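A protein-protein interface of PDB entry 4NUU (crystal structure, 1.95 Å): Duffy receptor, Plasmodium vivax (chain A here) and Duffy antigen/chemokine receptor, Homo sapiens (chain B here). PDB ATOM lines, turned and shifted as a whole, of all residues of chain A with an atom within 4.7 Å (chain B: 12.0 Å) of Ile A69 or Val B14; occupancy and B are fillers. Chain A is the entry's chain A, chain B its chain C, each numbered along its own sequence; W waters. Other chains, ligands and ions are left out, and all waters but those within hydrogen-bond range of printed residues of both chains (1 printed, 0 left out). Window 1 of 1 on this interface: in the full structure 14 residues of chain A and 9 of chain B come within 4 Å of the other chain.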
ATOM      1  N   LYS A  65     -20.942 -13.433  18.022  1.00  0.00           N
ATOM      2  CA  LYS A  65     -19.883 -14.056  18.799  1.00  0.00           C
ATOM      3  C   LYS A  65     -18.508 -13.630  18.282  1.00  0.00           C
ATOM      4  O   LYS A  65     -17.622 -13.292  19.062  1.00  0.00           O
ATOM      5  CB  LYS A  65     -20.028 -15.577  18.755  1.00  0.00           C
ATOM      6  CG  LYS A  65     -18.853 -16.329  19.337  1.00  0.00           C
ATOM      7  CD  LYS A  65     -18.908 -16.386  20.858  1.00  0.00           C
ATOM      8  CE  LYS A  65     -19.445 -17.728  21.345  1.00  0.00           C
ATOM      9  NZ  LYS A  65     -18.597 -18.871  20.897  1.00  0.00           N
ATOM     10  N   ARG A  66     -18.337 -13.629  16.964  1.00  0.00           N
ATOM     11  CA  ARG A  66     -17.052 -13.278  16.369  1.00  0.00           C
ATOM     12  C   ARG A  66     -16.691 -11.829  16.676  1.00  0.00           C
ATOM     13  O   ARG A  66     -15.562 -11.526  17.067  1.00  0.00           O
ATOM     14  CB  ARG A  66     -17.090 -13.510  14.863  1.00  0.00           C
ATOM     15  CG  ARG A  66     -17.663 -14.865  14.508  1.00  0.00           C
ATOM     16  CD  ARG A  66     -17.087 -15.428  13.237  1.00  0.00           C
ATOM     17  NE  ARG A  66     -17.145 -16.887  13.252  1.00  0.00           N
ATOM     18  CZ  ARG A  66     -16.433 -17.678  12.452  1.00  0.00           C
ATOM     19  NH1 ARG A  66     -15.601 -17.162  11.554  1.00  0.00           N
ATOM     20  NH2 ARG A  66     -16.543 -18.995  12.538  1.00  0.00           N
ATOM     21  N   LYS A  67     -17.663 -10.940  16.509  1.00  0.00           N
ATOM     22  CA  LYS A  67     -17.464  -9.520  16.765  1.00  0.00           C
ATOM     23  C   LYS A  67     -17.135  -9.261  18.234  1.00  0.00           C
ATOM     24  O   LYS A  67     -16.269  -8.444  18.560  1.00  0.00           O
ATOM     25  CB  LYS A  67     -18.716  -8.737  16.362  1.00  0.00           C
ATOM     26  CG  LYS A  67     -19.040  -8.810  14.875  1.00  0.00           C
ATOM     27  CD  LYS A  67     -17.805  -8.545  14.029  1.00  0.00           C
ATOM     28  CE  LYS A  67     -18.104  -8.606  12.546  1.00  0.00           C
ATOM     29  NZ  LYS A  67     -16.884  -8.296  11.747  1.00  0.00           N
ATOM     30  N   LEU A  68     -17.830  -9.960  19.123  1.00  0.00           N
ATOM     31  CA  LEU A  68     -17.645  -9.765  20.556  1.00  0.00           C
ATOM     32  C   LEU A  68     -16.275 -10.287  20.982  1.00  0.00           C
ATOM     33  O   LEU A  68     -15.574  -9.654  21.771  1.00  0.00           O
ATOM     34  CB  LEU A  68     -18.754 -10.477  21.328  1.00  0.00           C
ATOM     35  CG  LEU A  68     -18.738 -10.337  22.851  1.00  0.00           C
ATOM     36  CD1 LEU A  68     -18.855  -8.881  23.280  1.00  0.00           C
ATOM     37  CD2 LEU A  68     -19.865 -11.160  23.452  1.00  0.00           C
ATOM     38  N   ILE A  69     -15.901 -11.446  20.450  1.00  0.00           N
ATOM     39  CA  ILE A  69     -14.586 -12.016  20.698  1.00  0.00           C
ATOM     40  C   ILE A  69     -13.498 -11.025  20.312  1.00  0.00           C
ATOM     41  O   ILE A  69     -12.518 -10.853  21.037  1.00  0.00           O
ATOM     42  CB  ILE A  69     -14.375 -13.314  19.897  1.00  0.00           C
ATOM     43  CG1 ILE A  69     -15.158 -14.467  20.530  1.00  0.00           C
ATOM     44  CG2 ILE A  69     -12.894 -13.664  19.827  1.00  0.00           C
ATOM     45  CD1 ILE A  69     -14.561 -14.984  21.824  1.00  0.00           C
ATOM     46  N   TYR A  70     -13.668 -10.367  19.171  1.00  0.00           N
ATOM     47  CA  TYR A  70     -12.641  -9.455  18.692  1.00  0.00           C
ATOM     48  C   TYR A  70     -12.596  -8.148  19.499  1.00  0.00           C
ATOM     49  O   TYR A  70     -11.516  -7.669  19.845  1.00  0.00           O
ATOM     50  CB  TYR A  70     -12.798  -9.172  17.198  1.00  0.00           C
ATOM     51  CG  TYR A  70     -11.562  -8.534  16.613  1.00  0.00           C
ATOM     52  CD1 TYR A  70     -10.418  -9.286  16.382  1.00  0.00           C
ATOM     53  CD2 TYR A  70     -11.526  -7.178  16.314  1.00  0.00           C
ATOM     54  CE1 TYR A  70      -9.277  -8.711  15.861  1.00  0.00           C
ATOM     55  CE2 TYR A  70     -10.389  -6.593  15.791  1.00  0.00           C
ATOM     56  CZ  TYR A  70      -9.268  -7.363  15.566  1.00  0.00           C
ATOM     57  OH  TYR A  70      -8.132  -6.787  15.045  1.00  0.00           O
ATOM     58  N   ASP A  71     -13.752  -7.571  19.806  1.00  0.00           N
ATOM     59  CA  ASP A  71     -13.774  -6.370  20.639  1.00  0.00           C
ATOM     60  C   ASP A  71     -13.184  -6.670  22.017  1.00  0.00           C
ATOM     61  O   ASP A  71     -12.485  -5.844  22.598  1.00  0.00           O
ATOM     62  CB  ASP A  71     -15.196  -5.821  20.789  1.00  0.00           C
ATOM     63  CG  ASP A  71     -15.655  -5.032  19.570  1.00  0.00           C
ATOM     64  OD1 ASP A  71     -14.801  -4.642  18.742  1.00  0.00           O
ATOM     65  OD2 ASP A  71     -16.874  -4.789  19.444  1.00  0.00           O
ATOM     66  N   ALA A  72     -13.464  -7.861  22.532  1.00  0.00           N
ATOM     67  CA  ALA A  72     -12.990  -8.250  23.853  1.00  0.00           C
ATOM     68  C   ALA A  72     -11.471  -8.418  23.878  1.00  0.00           C
ATOM     69  O   ALA A  72     -10.808  -7.997  24.828  1.00  0.00           O
ATOM     70  CB  ALA A  72     -13.677  -9.531  24.302  1.00  0.00           C
ATOM     71  N   ALA A  73     -10.918  -9.026  22.832  1.00  0.00           N
ATOM     72  CA  ALA A  73      -9.476  -9.221  22.741  1.00  0.00           C
ATOM     73  C   ALA A  73      -8.738  -7.886  22.654  1.00  0.00           C
ATOM     74  O   ALA A  73      -7.661  -7.725  23.233  1.00  0.00           O
ATOM     75  CB  ALA A  73      -9.129 -10.093  21.542  1.00  0.00           C
ATOM     76  N   GLN A 148     -15.458 -17.974  27.062  1.00  0.00           N
ATOM     77  CA  GLN A 148     -14.677 -17.752  25.851  1.00  0.00           C
ATOM     78  C   GLN A 148     -14.360 -16.269  25.669  1.00  0.00           C
ATOM     79  O   GLN A 148     -13.289 -15.909  25.182  1.00  0.00           O
ATOM     80  CB  GLN A 148     -15.424 -18.296  24.633  1.00  0.00           C
ATOM     81  CG  GLN A 148     -15.684 -19.792  24.708  1.00  0.00           C
ATOM     82  CD  GLN A 148     -16.931 -20.210  23.956  1.00  0.00           C
ATOM     83  OE1 GLN A 148     -17.418 -19.491  23.085  1.00  0.00           O
ATOM     84  NE2 GLN A 148     -17.461 -21.381  24.298  1.00  0.00           N
ATOM     85  N   ILE A 149     -15.285 -15.406  26.074  1.00  0.00           N
ATOM     86  CA  ILE A 149     -15.045 -13.968  25.995  1.00  0.00           C
ATOM     87  C   ILE A 149     -13.920 -13.565  26.954  1.00  0.00           C
ATOM     88  O   ILE A 149     -13.036 -12.790  26.592  1.00  0.00           O
ATOM     89  CB  ILE A 149     -16.326 -13.154  26.279  1.00  0.00           C
ATOM     90  CG1 ILE A 149     -17.439 -13.545  25.305  1.00  0.00           C
ATOM     91  CG2 ILE A 149     -16.053 -11.665  26.147  1.00  0.00           C
ATOM     92  CD1 ILE A 149     -17.020 -13.514  23.849  1.00  0.00           C
ATOM     93  N   ALA A 152     -10.694 -14.608  25.461  1.00  0.00           N
ATOM     94  CA  ALA A 152     -10.319 -13.686  24.394  1.00  0.00           C
ATOM     95  C   ALA A 152      -9.652 -12.419  24.946  1.00  0.00           C
ATOM     96  O   ALA A 152      -8.714 -11.890  24.352  1.00  0.00           O
ATOM     97  CB  ALA A 152     -11.542 -13.322  23.567  1.00  0.00           C
ATOM     98  N   TYR A 155      -6.051 -12.819  25.516  1.00  0.00           N
ATOM     99  CA  TYR A 155      -5.266 -13.209  24.348  1.00  0.00           C
ATOM    100  C   TYR A 155      -3.834 -12.669  24.388  1.00  0.00           C
ATOM    101  O   TYR A 155      -2.880 -13.430  24.294  1.00  0.00           O
ATOM    102  CB  TYR A 155      -5.946 -12.751  23.056  1.00  0.00           C
ATOM    103  CG  TYR A 155      -5.096 -12.992  21.828  1.00  0.00           C
ATOM    104  CD1 TYR A 155      -5.040 -14.245  21.234  1.00  0.00           C
ATOM    105  CD2 TYR A 155      -4.339 -11.969  21.272  1.00  0.00           C
ATOM    106  CE1 TYR A 155      -4.260 -14.471  20.113  1.00  0.00           C
ATOM    107  CE2 TYR A 155      -3.557 -12.185  20.155  1.00  0.00           C
ATOM    108  CZ  TYR A 155      -3.520 -13.435  19.580  1.00  0.00           C
ATOM    109  OH  TYR A 155      -2.735 -13.643  18.466  1.00  0.00           O
ATOM    110  N   GLN B   8      -4.568  -4.474  15.403  1.00  0.00           N
ATOM    111  CA  GLN B   8      -3.341  -5.172  15.041  1.00  0.00           C
ATOM    112  C   GLN B   8      -3.410  -6.644  15.449  1.00  0.00           C
ATOM    113  O   GLN B   8      -2.493  -7.417  15.170  1.00  0.00           O
ATOM    114  CB  GLN B   8      -2.136  -4.498  15.698  1.00  0.00           C
ATOM    115  CG  GLN B   8      -0.793  -4.927  15.129  1.00  0.00           C
ATOM    116  CD  GLN B   8       0.155  -3.759  14.938  1.00  0.00           C
ATOM    117  OE1 GLN B   8       1.187  -3.666  15.602  1.00  0.00           O
ATOM    118  NE2 GLN B   8      -0.190  -2.862  14.022  1.00  0.00           N
ATOM    119  N   LEU B   9      -4.501  -7.023  16.108  1.00  0.00           N
ATOM    120  CA  LEU B   9      -4.704  -8.408  16.514  1.00  0.00           C
ATOM    121  C   LEU B   9      -5.274  -9.221  15.354  1.00  0.00           C
ATOM    122  O   LEU B   9      -6.190  -8.776  14.662  1.00  0.00           O
ATOM    123  CB  LEU B   9      -5.649  -8.482  17.719  1.00  0.00           C
ATOM    124  CG  LEU B   9      -5.177  -7.790  19.002  1.00  0.00           C
ATOM    125  CD1 LEU B   9      -6.253  -7.864  20.071  1.00  0.00           C
ATOM    126  CD2 LEU B   9      -3.882  -8.402  19.512  1.00  0.00           C
ATOM    127  N   ASP B  10      -4.722 -10.410  15.145  1.00  0.00           N
ATOM    128  CA  ASP B  10      -5.171 -11.291  14.074  1.00  0.00           C
ATOM    129  C   ASP B  10      -6.422 -12.041  14.510  1.00  0.00           C
ATOM    130  O   ASP B  10      -6.363 -12.890  15.401  1.00  0.00           O
ATOM    131  CB  ASP B  10      -4.066 -12.284  13.706  1.00  0.00           C
ATOM    132  CG  ASP B  10      -4.481 -13.233  12.598  1.00  0.00           C
ATOM    133  OD1 ASP B  10      -4.464 -12.815  11.422  1.00  0.00           O
ATOM    134  OD2 ASP B  10      -4.819 -14.397  12.901  1.00  0.00           O
ATOM    135  N   PHE B  11      -7.553 -11.729  13.884  1.00  0.00           N
ATOM    136  CA  PHE B  11      -8.822 -12.322  14.287  1.00  0.00           C
ATOM    137  C   PHE B  11      -8.753 -13.844  14.339  1.00  0.00           C
ATOM    138  O   PHE B  11      -9.170 -14.456  15.320  1.00  0.00           O
ATOM    139  CB  PHE B  11      -9.954 -11.911  13.348  1.00  0.00           C
ATOM    140  CG  PHE B  11     -11.236 -12.644  13.616  1.00  0.00           C
ATOM    141  CD1 PHE B  11     -12.073 -12.245  14.645  1.00  0.00           C
ATOM    142  CD2 PHE B  11     -11.590 -13.748  12.857  1.00  0.00           C
ATOM    143  CE1 PHE B  11     -13.247 -12.926  14.904  1.00  0.00           C
ATOM    144  CE2 PHE B  11     -12.762 -14.432  13.111  1.00  0.00           C
ATOM    145  CZ  PHE B  11     -13.591 -14.021  14.135  1.00  0.00           C
ATOM    146  N   GLU B  12      -8.235 -14.453  13.277  1.00  0.00           N
ATOM    147  CA  GLU B  12      -8.165 -15.907  13.203  1.00  0.00           C
ATOM    148  C   GLU B  12      -7.431 -16.479  14.413  1.00  0.00           C
ATOM    149  O   GLU B  12      -7.895 -17.429  15.041  1.00  0.00           O
ATOM    150  CB  GLU B  12      -7.475 -16.347  11.914  1.00  0.00           C
ATOM    151  CG  GLU B  12      -7.417 -17.856  11.734  1.00  0.00           C
ATOM    152  CD  GLU B  12      -6.783 -18.257  10.417  1.00  0.00           C
ATOM    153  OE1 GLU B  12      -7.530 -18.502   9.446  1.00  0.00           O
ATOM    154  OE2 GLU B  12      -5.540 -18.326  10.353  1.00  0.00           O
ATOM    155  N   ASP B  13      -6.284 -15.899  14.744  1.00  0.00           N
ATOM    156  CA  ASP B  13      -5.497 -16.397  15.864  1.00  0.00           C
ATOM    157  C   ASP B  13      -6.237 -16.166  17.179  1.00  0.00           C
ATOM    158  O   ASP B  13      -6.176 -16.994  18.088  1.00  0.00           O
ATOM    159  CB  ASP B  13      -4.126 -15.726  15.902  1.00  0.00           C
ATOM    160  CG  ASP B  13      -3.174 -16.406  16.868  1.00  0.00           C
ATOM    161  OD1 ASP B  13      -3.180 -17.655  16.925  1.00  0.00           O
ATOM    162  OD2 ASP B  13      -2.422 -15.697  17.570  1.00  0.00           O
ATOM    163  N   VAL B  14      -6.939 -15.040  17.273  1.00  0.00           N
ATOM    164  CA  VAL B  14      -7.731 -14.729  18.460  1.00  0.00           C
ATOM    165  C   VAL B  14      -8.881 -15.718  18.615  1.00  0.00           C
ATOM    166  O   VAL B  14      -9.119 -16.247  19.703  1.00  0.00           O
ATOM    167  CB  VAL B  14      -8.309 -13.303  18.399  1.00  0.00           C
ATOM    168  CG1 VAL B  14      -9.335 -13.092  19.504  1.00  0.00           C
ATOM    169  CG2 VAL B  14      -7.193 -12.269  18.502  1.00  0.00           C
ATOM    170  N   TRP B  15      -9.595 -15.958  17.521  1.00  0.00           N
ATOM    171  CA  TRP B  15     -10.717 -16.885  17.522  1.00  0.00           C
ATOM    172  C   TRP B  15     -10.285 -18.267  17.990  1.00  0.00           C
ATOM    173  O   TRP B  15     -10.916 -18.863  18.860  1.00  0.00           O
ATOM    174  CB  TRP B  15     -11.323 -16.985  16.121  1.00  0.00           C
ATOM    175  CG  TRP B  15     -12.381 -18.038  16.001  1.00  0.00           C
ATOM    176  CD1 TRP B  15     -12.219 -19.311  15.544  1.00  0.00           C
ATOM    177  CD2 TRP B  15     -13.764 -17.907  16.343  1.00  0.00           C
ATOM    178  NE1 TRP B  15     -13.416 -19.984  15.579  1.00  0.00           N
ATOM    179  CE2 TRP B  15     -14.382 -19.144  16.069  1.00  0.00           C
ATOM    180  CE3 TRP B  15     -14.543 -16.864  16.857  1.00  0.00           C
ATOM    181  CZ2 TRP B  15     -15.740 -19.369  16.290  1.00  0.00           C
ATOM    182  CZ3 TRP B  15     -15.892 -17.088  17.077  1.00  0.00           C
ATOM    183  CH2 TRP B  15     -16.477 -18.329  16.789  1.00  0.00           C
ATOM    184  N   ASN B  16      -9.203 -18.772  17.411  1.00  0.00           N
ATOM    185  CA  ASN B  16      -8.743 -20.122  17.707  1.00  0.00           C
ATOM    186  C   ASN B  16      -8.072 -20.232  19.076  1.00  0.00           C
ATOM    187  O   ASN B  16      -7.961 -21.320  19.635  1.00  0.00           O
ATOM    188  CB  ASN B  16      -7.802 -20.612  16.602  1.00  0.00           C
ATOM    189  CG  ASN B  16      -8.518 -20.806  15.278  1.00  0.00           C
ATOM    190  OD1 ASN B  16      -9.641 -21.305  15.245  1.00  0.00           O
ATOM    191  ND2 ASN B  16      -7.877 -20.405  14.182  1.00  0.00           N
ATOM    192  N   SER B  17      -7.633 -19.105  19.618  1.00  0.00           N
ATOM    193  CA  SER B  17      -6.999 -19.093  20.931  1.00  0.00           C
ATOM    194  C   SER B  17      -8.045 -19.053  22.046  1.00  0.00           C
ATOM    195  O   SER B  17      -7.774 -19.442  23.183  1.00  0.00           O
ATOM    196  CB  SER B  17      -6.062 -17.887  21.049  1.00  0.00           C
ATOM    197  OG  SER B  17      -5.341 -17.917  22.268  1.00  0.00           O
ATOM    198  N   SER B  18      -9.245 -18.593  21.707  1.00  0.00           N
ATOM    199  CA  SER B  18     -10.294 -18.363  22.695  1.00  0.00           C
ATOM    200  C   SER B  18     -11.051 -19.634  23.092  1.00  0.00           C
ATOM    201  O   SER B  18     -11.955 -19.583  23.927  1.00  0.00           O
ATOM    202  CB  SER B  18     -11.281 -17.326  22.163  1.00  0.00           C
ATOM    203  OG  SER B  18     -10.600 -16.162  21.731  1.00  0.00           O
ATOM    204  N   TYR B  19     -10.683 -20.767  22.501  1.00  0.00           N
ATOM    205  CA  TYR B  19     -11.331 -22.037  22.823  1.00  0.00           C
ATOM    206  C   TYR B  19     -10.322 -23.076  23.290  1.00  0.00           C
ATOM    207  O   TYR B  19     -10.415 -23.577  24.410  1.00  0.00           O
ATOM    208  CB  TYR B  19     -12.102 -22.559  21.610  1.00  0.00           C
ATOM    209  CG  TYR B  19     -13.219 -21.639  21.185  1.00  0.00           C
ATOM    210  CD1 TYR B  19     -12.966 -20.542  20.375  1.00  0.00           C
ATOM    211  CD2 TYR B  19     -14.523 -21.860  21.603  1.00  0.00           C
ATOM    212  CE1 TYR B  19     -13.981 -19.691  19.986  1.00  0.00           C
ATOM    213  CE2 TYR B  19     -15.546 -21.016  21.220  1.00  0.00           C
ATOM    214  CZ  TYR B  19     -15.267 -19.933  20.413  1.00  0.00           C
ATOM    215  OH  TYR B  19     -16.281 -19.089  20.030  1.00  0.00           O
HETATM  216  O   HOH W   1      -2.493 -11.215  16.657  1.00  0.00           O
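Of the 13 printed residues of chain A, 8 touch a printed residue of chain B.
Of the 12 printed residues of chain B, 8 touch a printed residue of chain A.
Printed residues of chain B that touch a printed residue of chain A: Leu B9, Phe B11, Asp B13, Val B14, Trp B15, Ser B17, Ser B18 and Tyr B19.
Hydrophobic or aromatic side chains of chain B within 4 Å of the printed part of chain A: Leu B9, Phe B11, Val B14, Trp B15 and Tyr B19.
Among the printed residues, no Asp or Glu carboxylate lies within 4 Å of a Lys or Arg side-chain nitrogen of the other chain.
The side-chain hydroxyl of Tyr B19 sits at hydrogen-bond distance from the side-chain amino group of Lys A65 (2.5 Å).
O of Leu B9 sits at hydrogen-bond distance from OH of Tyr A70 (2.8 Å).
OE1 of Gln A148 lies close to OH of Tyr B19, at 3.3 Å.
The side-chain hydroxyl (OH) of Tyr A155 lies close to the side-chain carboxylate (OD2) of Asp B13.
The side-chain amide oxygen of Gln A148 lies within hydrogen-bond range of the side-chain amino group of Lys A65 (2.6 Å).
OD2 of Asp B10 is in hydrogen-bond range of N of Asp B13, 2.8 Å away.
O of Val B14 is in hydrogen-bond range of OG of Ser B18 (2.5 Å).
O of Arg A66 touches CE1 of Phe B11 (3.5 Å).
Trp B15 touches Arg A66 (CZ3 to CG, 3.8 Å).
CG1 of Val B14 touches CG2 of Ile A69 (3.6 Å).
Ser B18 touches Ile A69 (OG to CG2, 3.9 Å).
Tyr A70 touches Phe B11 (CD1 to CD1, 3.8 Å).
O of Ala A73 touches CD1 of Leu B9, 3.5 Å away.
Gln A148 touches Ser B18 (CB to O, 3.8 Å).
Leu B9 touches Tyr A155 (CD2 to CE2, 3.9 Å).
CE1 of Tyr A155 touches CA of Val B14, at 3.9 Å.
CB of Ser B17 touches CD1 of Tyr A155, 3.8 Å away.
Water W1 lies within hydrogen-bond range of N of Asp B10 (2.8 Å) and OH of Tyr A155 (3.0 Å).
No residue of chain B comes within 4 Å of Leu A68.
Ile A69 touches just these residues of chain B: Val B14 and Ser B18.
No residue of chain B comes within 4 Å of Asp A71.
No residue of chain B comes within 4 Å of Ala A72.
Ala A152 touches one residue of chain B.
Of the printed residues of chain A, Phe B11 touches Arg A66 and Tyr A70.
Glu B12 touches none of the printed residues of chain A.
Printed residues of chain A within 4 Å of Asp B13: Tyr A155.
Printed residues of chain A within 4 Å of Trp B15: Lys A65 and Arg A66.
Printed residues of chain A within 4 Å of Tyr B19: Lys A65 and Gln A148.
The nearest residue of chain A that does not touch Val B14 is Ala A152 (4.6 Å).
The nearest printed residue of chain A that does not touch Tyr B19 is Ile A69 (4.8 Å).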
